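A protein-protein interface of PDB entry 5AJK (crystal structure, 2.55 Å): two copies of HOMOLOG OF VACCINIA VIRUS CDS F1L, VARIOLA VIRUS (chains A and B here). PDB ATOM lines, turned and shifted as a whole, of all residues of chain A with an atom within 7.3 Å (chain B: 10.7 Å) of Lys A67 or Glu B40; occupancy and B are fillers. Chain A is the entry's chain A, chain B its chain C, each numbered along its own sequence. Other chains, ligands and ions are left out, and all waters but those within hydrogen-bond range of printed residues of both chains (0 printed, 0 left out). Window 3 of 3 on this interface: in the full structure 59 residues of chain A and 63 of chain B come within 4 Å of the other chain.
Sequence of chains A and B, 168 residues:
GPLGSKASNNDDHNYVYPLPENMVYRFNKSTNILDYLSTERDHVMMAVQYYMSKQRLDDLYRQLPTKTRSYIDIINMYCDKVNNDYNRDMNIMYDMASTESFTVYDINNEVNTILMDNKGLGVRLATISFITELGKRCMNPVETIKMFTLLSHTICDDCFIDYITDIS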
ATOM      1  N   LEU A  64     -36.593   7.479  24.706  1.00  0.00           N
ATOM      2  CA  LEU A  64     -35.281   8.051  24.985  1.00  0.00           C
ATOM      3  C   LEU A  64     -34.315   6.956  25.432  1.00  0.00           C
ATOM      4  O   LEU A  64     -34.666   6.137  26.283  1.00  0.00           O
ATOM      5  CB  LEU A  64     -35.370   9.147  26.052  1.00  0.00           C
ATOM      6  CG  LEU A  64     -36.044  10.475  25.680  1.00  0.00           C
ATOM      7  CD1 LEU A  64     -35.821  11.501  26.784  1.00  0.00           C
ATOM      8  CD2 LEU A  64     -35.556  11.019  24.341  1.00  0.00           C
ATOM      9  N   PRO A  65     -33.095   6.931  24.858  1.00  0.00           N
ATOM     10  CA  PRO A  65     -32.089   5.945  25.277  1.00  0.00           C
ATOM     11  C   PRO A  65     -31.801   5.997  26.774  1.00  0.00           C
ATOM     12  O   PRO A  65     -32.106   6.998  27.422  1.00  0.00           O
ATOM     13  CB  PRO A  65     -30.844   6.347  24.479  1.00  0.00           C
ATOM     14  CG  PRO A  65     -31.359   7.081  23.309  1.00  0.00           C
ATOM     15  CD  PRO A  65     -32.596   7.784  23.763  1.00  0.00           C
ATOM     16  N   THR A  66     -31.212   4.931  27.308  1.00  0.00           N
ATOM     17  CA  THR A  66     -30.871   4.866  28.724  1.00  0.00           C
ATOM     18  C   THR A  66     -29.920   6.005  29.093  1.00  0.00           C
ATOM     19  O   THR A  66     -29.905   6.484  30.229  1.00  0.00           O
ATOM     20  CB  THR A  66     -30.235   3.489  29.081  1.00  0.00           C
ATOM     21  OG1 THR A  66     -30.806   2.989  30.295  1.00  0.00           O
ATOM     22  CG2 THR A  66     -28.710   3.577  29.234  1.00  0.00           C
ATOM     23  N   LYS A  67     -29.143   6.443  28.111  1.00  0.00           N
ATOM     24  CA  LYS A  67     -28.120   7.458  28.317  1.00  0.00           C
ATOM     25  C   LYS A  67     -28.729   8.843  28.524  1.00  0.00           C
ATOM     26  O   LYS A  67     -28.305   9.590  29.406  1.00  0.00           O
ATOM     27  CB  LYS A  67     -27.170   7.477  27.122  1.00  0.00           C
ATOM     28  CG  LYS A  67     -25.960   8.379  27.272  1.00  0.00           C
ATOM     29  CD  LYS A  67     -25.143   8.371  25.993  1.00  0.00           C
ATOM     30  CE  LYS A  67     -23.809   9.063  26.172  1.00  0.00           C
ATOM     31  NZ  LYS A  67     -22.983   8.964  24.937  1.00  0.00           N
ATOM     32  N   THR A  68     -29.716   9.181  27.698  1.00  0.00           N
ATOM     33  CA  THR A  68     -30.388  10.470  27.805  1.00  0.00           C
ATOM     34  C   THR A  68     -31.117  10.569  29.136  1.00  0.00           C
ATOM     35  O   THR A  68     -31.127  11.620  29.771  1.00  0.00           O
ATOM     36  CB  THR A  68     -31.396  10.686  26.660  1.00  0.00           C
ATOM     37  OG1 THR A  68     -30.850  10.184  25.438  1.00  0.00           O
ATOM     38  CG2 THR A  68     -31.715  12.164  26.496  1.00  0.00           C
ATOM     39  N   ARG A  69     -31.717   9.461  29.556  1.00  0.00           N
ATOM     40  CA  ARG A  69     -32.484   9.425  30.794  1.00  0.00           C
ATOM     41  C   ARG A  69     -31.609   9.712  32.008  1.00  0.00           C
ATOM     42  O   ARG A  69     -32.082  10.257  33.006  1.00  0.00           O
ATOM     43  CB  ARG A  69     -33.171   8.070  30.958  1.00  0.00           C
ATOM     44  CG  ARG A  69     -34.265   7.810  29.945  1.00  0.00           C
ATOM     45  CD  ARG A  69     -35.082   6.596  30.329  1.00  0.00           C
ATOM     46  NE  ARG A  69     -36.051   6.234  29.299  1.00  0.00           N
ATOM     47  CZ  ARG A  69     -37.020   5.341  29.466  1.00  0.00           C
ATOM     48  NH1 ARG A  69     -37.160   4.717  30.628  1.00  0.00           N
ATOM     49  NH2 ARG A  69     -37.853   5.073  28.473  1.00  0.00           N
ATOM     50  N   SER A  70     -30.333   9.350  31.918  1.00  0.00           N
ATOM     51  CA  SER A  70     -29.404   9.577  33.015  1.00  0.00           C
ATOM     52  C   SER A  70     -28.993  11.040  33.057  1.00  0.00           C
ATOM     53  O   SER A  70     -28.727  11.586  34.126  1.00  0.00           O
ATOM     54  CB  SER A  70     -28.171   8.688  32.878  1.00  0.00           C
ATOM     55  OG  SER A  70     -27.334   9.145  31.832  1.00  0.00           O
ATOM     56  N   TYR A  71     -28.932  11.671  31.889  1.00  0.00           N
ATOM     57  CA  TYR A  71     -28.678  13.105  31.823  1.00  0.00           C
ATOM     58  C   TYR A  71     -29.883  13.871  32.361  1.00  0.00           C
ATOM     59  O   TYR A  71     -29.728  14.911  32.999  1.00  0.00           O
ATOM     60  CB  TYR A  71     -28.366  13.543  30.390  1.00  0.00           C
ATOM     61  CG  TYR A  71     -27.055  13.020  29.846  1.00  0.00           C
ATOM     62  CD1 TYR A  71     -26.047  12.581  30.697  1.00  0.00           C
ATOM     63  CD2 TYR A  71     -26.825  12.970  28.480  1.00  0.00           C
ATOM     64  CE1 TYR A  71     -24.851  12.104  30.201  1.00  0.00           C
ATOM     65  CE2 TYR A  71     -25.630  12.493  27.974  1.00  0.00           C
ATOM     66  CZ  TYR A  71     -24.646  12.062  28.838  1.00  0.00           C
ATOM     67  OH  TYR A  71     -23.454  11.587  28.341  1.00  0.00           O
ATOM     68  N   ILE A  72     -31.079  13.352  32.102  1.00  0.00           N
ATOM     69  CA  ILE A  72     -32.294  13.937  32.651  1.00  0.00           C
ATOM     70  C   ILE A  72     -32.284  13.841  34.177  1.00  0.00           C
ATOM     71  O   ILE A  72     -32.633  14.799  34.867  1.00  0.00           O
ATOM     72  CB  ILE A  72     -33.552  13.247  32.091  1.00  0.00           C
ATOM     73  CG1 ILE A  72     -33.705  13.568  30.603  1.00  0.00           C
ATOM     74  CG2 ILE A  72     -34.798  13.703  32.842  1.00  0.00           C
ATOM     75  CD1 ILE A  72     -34.772  12.750  29.894  1.00  0.00           C
ATOM     76  N   ASP A  73     -31.887  12.682  34.694  1.00  0.00           N
ATOM     77  CA  ASP A  73     -31.796  12.473  36.137  1.00  0.00           C
ATOM     78  C   ASP A  73     -30.849  13.475  36.791  1.00  0.00           C
ATOM     79  O   ASP A  73     -31.139  14.012  37.860  1.00  0.00           O
ATOM     80  CB  ASP A  73     -31.326  11.049  36.444  1.00  0.00           C
ATOM     81  CG  ASP A  73     -32.433  10.018  36.306  1.00  0.00           C
ATOM     82  OD1 ASP A  73     -33.616  10.366  36.511  1.00  0.00           O
ATOM     83  OD2 ASP A  73     -32.116   8.850  36.000  1.00  0.00           O
ATOM     84  N   ILE A  74     -29.713  13.713  36.144  1.00  0.00           N
ATOM     85  CA  ILE A  74     -28.727  14.659  36.649  1.00  0.00           C
ATOM     86  C   ILE A  74     -29.306  16.068  36.655  1.00  0.00           C
ATOM     87  O   ILE A  74     -29.213  16.777  37.651  1.00  0.00           O
ATOM     88  CB  ILE A  74     -27.433  14.631  35.804  1.00  0.00           C
ATOM     89  CG1 ILE A  74     -26.728  13.283  35.964  1.00  0.00           C
ATOM     90  CG2 ILE A  74     -26.472  15.747  36.222  1.00  0.00           C
ATOM     91  CD1 ILE A  74     -25.729  12.976  34.869  1.00  0.00           C
ATOM     92  N   CYS A 156     -26.488  24.597  26.272  1.00  0.00           N
ATOM     93  CA  CYS A 156     -25.661  23.411  26.089  1.00  0.00           C
ATOM     94  C   CYS A 156     -24.461  23.683  25.186  1.00  0.00           C
ATOM     95  O   CYS A 156     -24.285  23.032  24.155  1.00  0.00           O
ATOM     96  CB  CYS A 156     -26.503  22.266  25.522  1.00  0.00           C
ATOM     97  SG  CYS A 156     -27.836  21.735  26.627  1.00  0.00           S
ATOM     98  N   ILE A 161     -21.724  20.689  28.289  1.00  0.00           N
ATOM     99  CA  ILE A 161     -21.780  19.255  28.028  1.00  0.00           C
ATOM    100  C   ILE A 161     -20.595  18.551  28.684  1.00  0.00           C
ATOM    101  O   ILE A 161     -20.693  17.389  29.069  1.00  0.00           O
ATOM    102  CB  ILE A 161     -21.810  18.942  26.513  1.00  0.00           C
ATOM    103  CG1 ILE A 161     -20.530  19.414  25.819  1.00  0.00           C
ATOM    104  CG2 ILE A 161     -23.025  19.597  25.872  1.00  0.00           C
ATOM    105  CD1 ILE A 161     -20.360  18.859  24.421  1.00  0.00           C
ATOM    106  N   ILE A 164     -21.618  17.926  32.295  1.00  0.00           N
ATOM    107  CA  ILE A 164     -22.637  16.882  32.408  1.00  0.00           C
ATOM    108  C   ILE A 164     -22.124  15.465  32.135  1.00  0.00           C
ATOM    109  O   ILE A 164     -22.568  14.515  32.778  1.00  0.00           O
ATOM    110  CB  ILE A 164     -23.807  17.152  31.443  1.00  0.00           C
ATOM    111  CG1 ILE A 164     -24.479  18.489  31.770  1.00  0.00           C
ATOM    112  CG2 ILE A 164     -24.831  16.024  31.500  1.00  0.00           C
ATOM    113  CD1 ILE A 164     -25.124  18.563  33.147  1.00  0.00           C
ATOM    114  N   THR A 165     -21.223  15.311  31.168  1.00  0.00           N
ATOM    115  CA  THR A 165     -20.718  13.982  30.821  1.00  0.00           C
ATOM    116  C   THR A 165     -19.655  13.495  31.808  1.00  0.00           C
ATOM    117  O   THR A 165     -19.296  12.318  31.804  1.00  0.00           O
ATOM    118  CB  THR A 165     -20.125  13.945  29.392  1.00  0.00           C
ATOM    119  OG1 THR A 165     -19.041  14.877  29.281  1.00  0.00           O
ATOM    120  CG2 THR A 165     -21.195  14.272  28.358  1.00  0.00           C
ATOM    121  N   SER A 168     -21.821  12.197  34.937  1.00  0.00           N
ATOM    122  CA  SER A 168     -22.443  10.924  34.582  1.00  0.00           C
ATOM    123  C   SER A 168     -21.423   9.790  34.662  1.00  0.00           C
ATOM    124  O   SER A 168     -21.787   8.615  34.711  1.00  0.00           O
ATOM    125  CB  SER A 168     -23.048  10.985  33.178  1.00  0.00           C
ATOM    126  OG  SER A 168     -22.040  11.126  32.191  1.00  0.00           O
ATOM    127  N   LEU B  34     -33.664   7.968  17.802  1.00  0.00           N
ATOM    128  CA  LEU B  34     -32.264   7.581  17.939  1.00  0.00           C
ATOM    129  C   LEU B  34     -31.394   8.148  16.822  1.00  0.00           C
ATOM    130  O   LEU B  34     -30.180   8.280  16.978  1.00  0.00           O
ATOM    131  CB  LEU B  34     -32.136   6.057  17.967  1.00  0.00           C
ATOM    132  CG  LEU B  34     -32.162   5.429  19.360  1.00  0.00           C
ATOM    133  CD1 LEU B  34     -32.526   3.958  19.280  1.00  0.00           C
ATOM    134  CD2 LEU B  34     -30.813   5.607  20.042  1.00  0.00           C
ATOM    135  N   ASP B  35     -32.019   8.481  15.697  1.00  0.00           N
ATOM    136  CA  ASP B  35     -31.300   9.042  14.558  1.00  0.00           C
ATOM    137  C   ASP B  35     -30.815  10.458  14.853  1.00  0.00           C
ATOM    138  O   ASP B  35     -29.787  10.893  14.334  1.00  0.00           O
ATOM    139  CB  ASP B  35     -32.187   9.047  13.311  1.00  0.00           C
ATOM    140  CG  ASP B  35     -32.507   7.649  12.813  1.00  0.00           C
ATOM    141  OD1 ASP B  35     -32.583   6.719  13.645  1.00  0.00           O
ATOM    142  OD2 ASP B  35     -32.682   7.481  11.588  1.00  0.00           O
ATOM    143  N   TYR B  36     -31.562  11.171  15.690  1.00  0.00           N
ATOM    144  CA  TYR B  36     -31.249  12.560  16.014  1.00  0.00           C
ATOM    145  C   TYR B  36     -30.308  12.666  17.211  1.00  0.00           C
ATOM    146  O   TYR B  36     -29.627  13.677  17.383  1.00  0.00           O
ATOM    147  CB  TYR B  36     -32.537  13.342  16.286  1.00  0.00           C
ATOM    148  CG  TYR B  36     -33.452  13.416  15.085  1.00  0.00           C
ATOM    149  CD1 TYR B  36     -34.248  12.336  14.731  1.00  0.00           C
ATOM    150  CD2 TYR B  36     -33.515  14.561  14.302  1.00  0.00           C
ATOM    151  CE1 TYR B  36     -35.081  12.392  13.632  1.00  0.00           C
ATOM    152  CE2 TYR B  36     -34.348  14.628  13.199  1.00  0.00           C
ATOM    153  CZ  TYR B  36     -35.130  13.540  12.870  1.00  0.00           C
ATOM    154  OH  TYR B  36     -35.961  13.600  11.774  1.00  0.00           O
ATOM    155  N   LEU B  37     -30.270  11.621  18.032  1.00  0.00           N
ATOM    156  CA  LEU B  37     -29.381  11.587  19.187  1.00  0.00           C
ATOM    157  C   LEU B  37     -28.027  11.002  18.803  1.00  0.00           C
ATOM    158  O   LEU B  37     -27.725   9.847  19.109  1.00  0.00           O
ATOM    159  CB  LEU B  37     -30.008  10.777  20.324  1.00  0.00           C
ATOM    160  CG  LEU B  37     -31.366  11.282  20.821  1.00  0.00           C
ATOM    161  CD1 LEU B  37     -31.890  10.382  21.925  1.00  0.00           C
ATOM    162  CD2 LEU B  37     -31.281  12.725  21.302  1.00  0.00           C
ATOM    163  N   SER B  38     -27.218  11.811  18.124  1.00  0.00           N
ATOM    164  CA  SER B  38     -25.906  11.381  17.654  1.00  0.00           C
ATOM    165  C   SER B  38     -24.810  11.761  18.643  1.00  0.00           C
ATOM    166  O   SER B  38     -24.267  10.904  19.341  1.00  0.00           O
ATOM    167  CB  SER B  38     -25.607  11.992  16.283  1.00  0.00           C
ATOM    168  OG  SER B  38     -26.607  11.639  15.342  1.00  0.00           O
ATOM    169  N   THR B  39     -24.494  13.050  18.698  1.00  0.00           N
ATOM    170  CA  THR B  39     -23.406  13.545  19.531  1.00  0.00           C
ATOM    171  C   THR B  39     -23.813  13.627  20.996  1.00  0.00           C
ATOM    172  O   THR B  39     -24.991  13.505  21.329  1.00  0.00           O
ATOM    173  CB  THR B  39     -22.943  14.938  19.075  1.00  0.00           C
ATOM    174  OG1 THR B  39     -23.969  15.901  19.352  1.00  0.00           O
ATOM    175  CG2 THR B  39     -22.638  14.940  17.588  1.00  0.00           C
ATOM    176  N   GLU B  40     -22.829  13.837  21.865  1.00  0.00           N
ATOM    177  CA  GLU B  40     -23.093  14.044  23.284  1.00  0.00           C
ATOM    178  C   GLU B  40     -23.964  15.278  23.491  1.00  0.00           C
ATOM    179  O   GLU B  40     -24.827  15.299  24.367  1.00  0.00           O
ATOM    180  CB  GLU B  40     -21.781  14.193  24.058  1.00  0.00           C
ATOM    181  CG  GLU B  40     -21.035  12.886  24.294  1.00  0.00           C
ATOM    182  CD  GLU B  40     -21.712  11.991  25.319  1.00  0.00           C
ATOM    183  OE1 GLU B  40     -22.751  12.396  25.880  1.00  0.00           O
ATOM    184  OE2 GLU B  40     -21.198  10.880  25.566  1.00  0.00           O
ATOM    185  N   ARG B  41     -23.734  16.300  22.671  1.00  0.00           N
ATOM    186  CA  ARG B  41     -24.474  17.554  22.764  1.00  0.00           C
ATOM    187  C   ARG B  41     -25.966  17.331  22.541  1.00  0.00           C
ATOM    188  O   ARG B  41     -26.799  17.900  23.246  1.00  0.00           O
ATOM    189  CB  ARG B  41     -23.938  18.563  21.747  1.00  0.00           C
ATOM    190  CG  ARG B  41     -24.559  19.946  21.847  1.00  0.00           C
ATOM    191  CD  ARG B  41     -23.932  20.907  20.850  1.00  0.00           C
ATOM    192  NE  ARG B  41     -24.346  22.289  21.095  1.00  0.00           N
ATOM    193  CZ  ARG B  41     -25.327  22.923  20.454  1.00  0.00           C
ATOM    194  NH1 ARG B  41     -26.023  22.321  19.495  1.00  0.00           N
ATOM    195  NH2 ARG B  41     -25.610  24.179  20.770  1.00  0.00           N
ATOM    196  N   ASP B  42     -26.293  16.496  21.560  1.00  0.00           N
ATOM    197  CA  ASP B  42     -27.683  16.178  21.251  1.00  0.00           C
ATOM    198  C   ASP B  42     -28.360  15.506  22.442  1.00  0.00           C
ATOM    199  O   ASP B  42     -29.530  15.760  22.726  1.00  0.00           O
ATOM    200  CB  ASP B  42     -27.766  15.271  20.018  1.00  0.00           C
ATOM    201  CG  ASP B  42     -27.285  15.956  18.750  1.00  0.00           C
ATOM    202  OD1 ASP B  42     -27.541  17.168  18.588  1.00  0.00           O
ATOM    203  OD2 ASP B  42     -26.652  15.279  17.913  1.00  0.00           O
ATOM    204  N   HIS B  43     -27.614  14.653  23.138  1.00  0.00           N
ATOM    205  CA  HIS B  43     -28.138  13.951  24.303  1.00  0.00           C
ATOM    206  C   HIS B  43     -28.433  14.911  25.452  1.00  0.00           C
ATOM    207  O   HIS B  43     -29.451  14.780  26.131  1.00  0.00           O
ATOM    208  CB  HIS B  43     -27.152  12.875  24.766  1.00  0.00           C
ATOM    209  CG  HIS B  43     -27.266  11.590  24.008  1.00  0.00           C
ATOM    210  ND1 HIS B  43     -28.115  10.575  24.392  1.00  0.00           N
ATOM    211  CD2 HIS B  43     -26.644  11.155  22.887  1.00  0.00           C
ATOM    212  CE1 HIS B  43     -28.011   9.569  23.542  1.00  0.00           C
ATOM    213  NE2 HIS B  43     -27.124   9.897  22.618  1.00  0.00           N
ATOM    214  N   VAL B  44     -27.541  15.873  25.668  1.00  0.00           N
ATOM    215  CA  VAL B  44     -27.697  16.823  26.761  1.00  0.00           C
ATOM    216  C   VAL B  44     -28.799  17.822  26.423  1.00  0.00           C
ATOM    217  O   VAL B  44     -29.608  18.174  27.280  1.00  0.00           O
ATOM    218  CB  VAL B  44     -26.376  17.565  27.061  1.00  0.00           C
ATOM    219  CG1 VAL B  44     -26.569  18.609  28.158  1.00  0.00           C
ATOM    220  CG2 VAL B  44     -25.296  16.579  27.473  1.00  0.00           C
ATOM    221  N   MET B  45     -28.830  18.270  25.170  1.00  0.00           N
ATOM    222  CA  MET B  45     -29.883  19.167  24.710  1.00  0.00           C
ATOM    223  C   MET B  45     -31.245  18.514  24.885  1.00  0.00           C
ATOM    224  O   MET B  45     -32.196  19.156  25.329  1.00  0.00           O
ATOM    225  CB  MET B  45     -29.679  19.549  23.243  1.00  0.00           C
ATOM    226  CG  MET B  45     -28.724  20.710  23.028  1.00  0.00           C
ATOM    227  SD  MET B  45     -28.792  21.369  21.350  1.00  0.00           S
ATOM    228  CE  MET B  45     -28.362  19.922  20.385  1.00  0.00           C
ATOM    229  N   MET B  46     -31.333  17.235  24.537  1.00  0.00           N
ATOM    230  CA  MET B  46     -32.583  16.499  24.669  1.00  0.00           C
ATOM    231  C   MET B  46     -33.002  16.467  26.133  1.00  0.00           C
ATOM    232  O   MET B  46     -34.163  16.706  26.458  1.00  0.00           O
ATOM    233  CB  MET B  46     -32.439  15.078  24.119  1.00  0.00           C
ATOM    234  CG  MET B  46     -33.717  14.244  24.176  1.00  0.00           C
ATOM    235  SD  MET B  46     -35.066  14.931  23.193  1.00  0.00           S
ATOM    236  CE  MET B  46     -34.394  14.739  21.545  1.00  0.00           C
ATOM    237  N   ALA B  47     -32.041  16.187  27.010  1.00  0.00           N
ATOM    238  CA  ALA B  47     -32.302  16.118  28.442  1.00  0.00           C
ATOM    239  C   ALA B  47     -32.802  17.460  28.972  1.00  0.00           C
ATOM    240  O   ALA B  47     -33.782  17.517  29.712  1.00  0.00           O
ATOM    241  CB  ALA B  47     -31.052  15.693  29.186  1.00  0.00           C
ATOM    242  N   VAL B  48     -32.120  18.534  28.586  1.00  0.00           N
ATOM    243  CA  VAL B  48     -32.505  19.881  28.995  1.00  0.00           C
ATOM    244  C   VAL B  48     -33.896  20.232  28.474  1.00  0.00           C
ATOM    245  O   VAL B  48     -34.746  20.705  29.229  1.00  0.00           O
ATOM    246  CB  VAL B  48     -31.481  20.931  28.498  1.00  0.00           C
ATOM    247  CG1 VAL B  48     -32.028  22.355  28.628  1.00  0.00           C
ATOM    248  CG2 VAL B  48     -30.176  20.803  29.269  1.00  0.00           C
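The side-chain amino group (NZ) of Lys A67 lies within salt-bridge range of the side-chain carboxylate (OE2) of Glu B40 (2.7 Å). OG1 of Thr A68 sits at hydrogen-bond distance from ND1 of His B43 (3.0 Å). NE of Arg B41 is in hydrogen-bond range of O of Cys A156, at 3.1 Å. OH of Tyr A71 lies within hydrogen-bond range of OE1 of Glu B40.
The side-chain hydroxyl of Ser A168 sits at hydrogen-bond distance from the backbone carbonyl oxygen of Thr A165 (3.0 Å). NH1 of Arg B41 lies within hydrogen-bond range of SD of Met B45, 3.5 Å away. The backbone carbonyl oxygen (O) of Ile A161 sits at hydrogen-bond distance from the side-chain hydroxyl (OG1) of Thr A165 (3.0 Å). NE of Arg A69 lies within hydrogen-bond range of O of Leu A64 (3.3 Å). The side-chain hydroxyl of Thr B39 sits close to the backbone NH of Arg B41, 3.4 Å away. The backbone carbonyl oxygen of Lys A67 is in hydrogen-bond range of the side-chain hydroxyl of Ser A70 (2.7 Å).
Among the printed residues, merely in contact across the chains: Pro A65 with Leu B37 (3.3 Å), Thr A165 with Glu B40 (3.5 Å), Tyr A71 with His B43 (3.6 Å), Ile A72 with Ala B47 (3.6 Å), Pro A65 with Leu B34 (3.6 Å), Tyr A71 with Ala B47 (3.6 Å), Cys A156 with Val B48 (3.7 Å), Thr A68 with Leu B37 (3.7 Å), Cys A156 with Met B45 (3.7 Å), Thr A68 with Met B46 (3.7 Å), Cys A156 with Val B44 (3.7 Å), Leu A64 with Met B46 (3.7 Å), Lys A67 with His B43 (3.96 Å) and Ile A161 with Arg B41 (3.99 Å).
Lys A67 touches just these residues of chain B: Glu B40 (2.7 Å) and His B43 (3.96 Å). Of chain A, only Lys A67, Tyr A71 and Thr A165 come within 4 Å of Glu B40. Of chain B, only Leu B37, His B43 and Met B46 come within 4 Å of Thr A68. No residue of chain B comes within 4 Å of Ser A70. Printed residues of chain B within 4 Å of Ile A72: Ala B47. Of the printed residues of chain A, His B43 touches Lys A67 (3.96 Å), Thr A68 (3.0 Å) and Tyr A71 (3.6 Å). Printed residues of chain A within 4 Å of Val B48: Cys A156 (3.7 Å). Of the printed residues of chain B, Cys A156 touches Arg B41, Val B44, Met B45 and Val B48. Printed residues of chain A within 4 Å of Ala B47: Tyr A71 (3.6 Å) and Ile A72 (3.6 Å). Tyr B36 touches none of the printed residues of chain A. Ser A168 touches none of the printed residues of chain B. The nearest residue of chain B that does not touch Lys A67 is Ser B38 (6.1 Å). The nearest printed residue of chain A that does not touch Met B46 is Ile A72 (5.2 Å).
Hydrophobic or aromatic side chains of chain A within 4 Å of the printed part of chain B: Leu A64, Pro A65, Tyr A71, Ile A72 and Ile A161. Along chain A the printed residues that touch a printed residue of chain B span positions 64 to 165. Of the 15 printed residues of chain B, 10 touch a printed residue of chain A. Along chain B the printed residues that touch a printed residue of chain A span positions 34 to 48. Among the printed residues, Asp or Glu carboxylates within 4 Å of a Lys or Arg side-chain nitrogen of the other chain: Lys A67 with Glu B40 (2.7 Å).
No position is printed for both chains. Of the 18 pairs that touch across the chains among the printed residues, none has its exchanged pair printed and touching as well.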
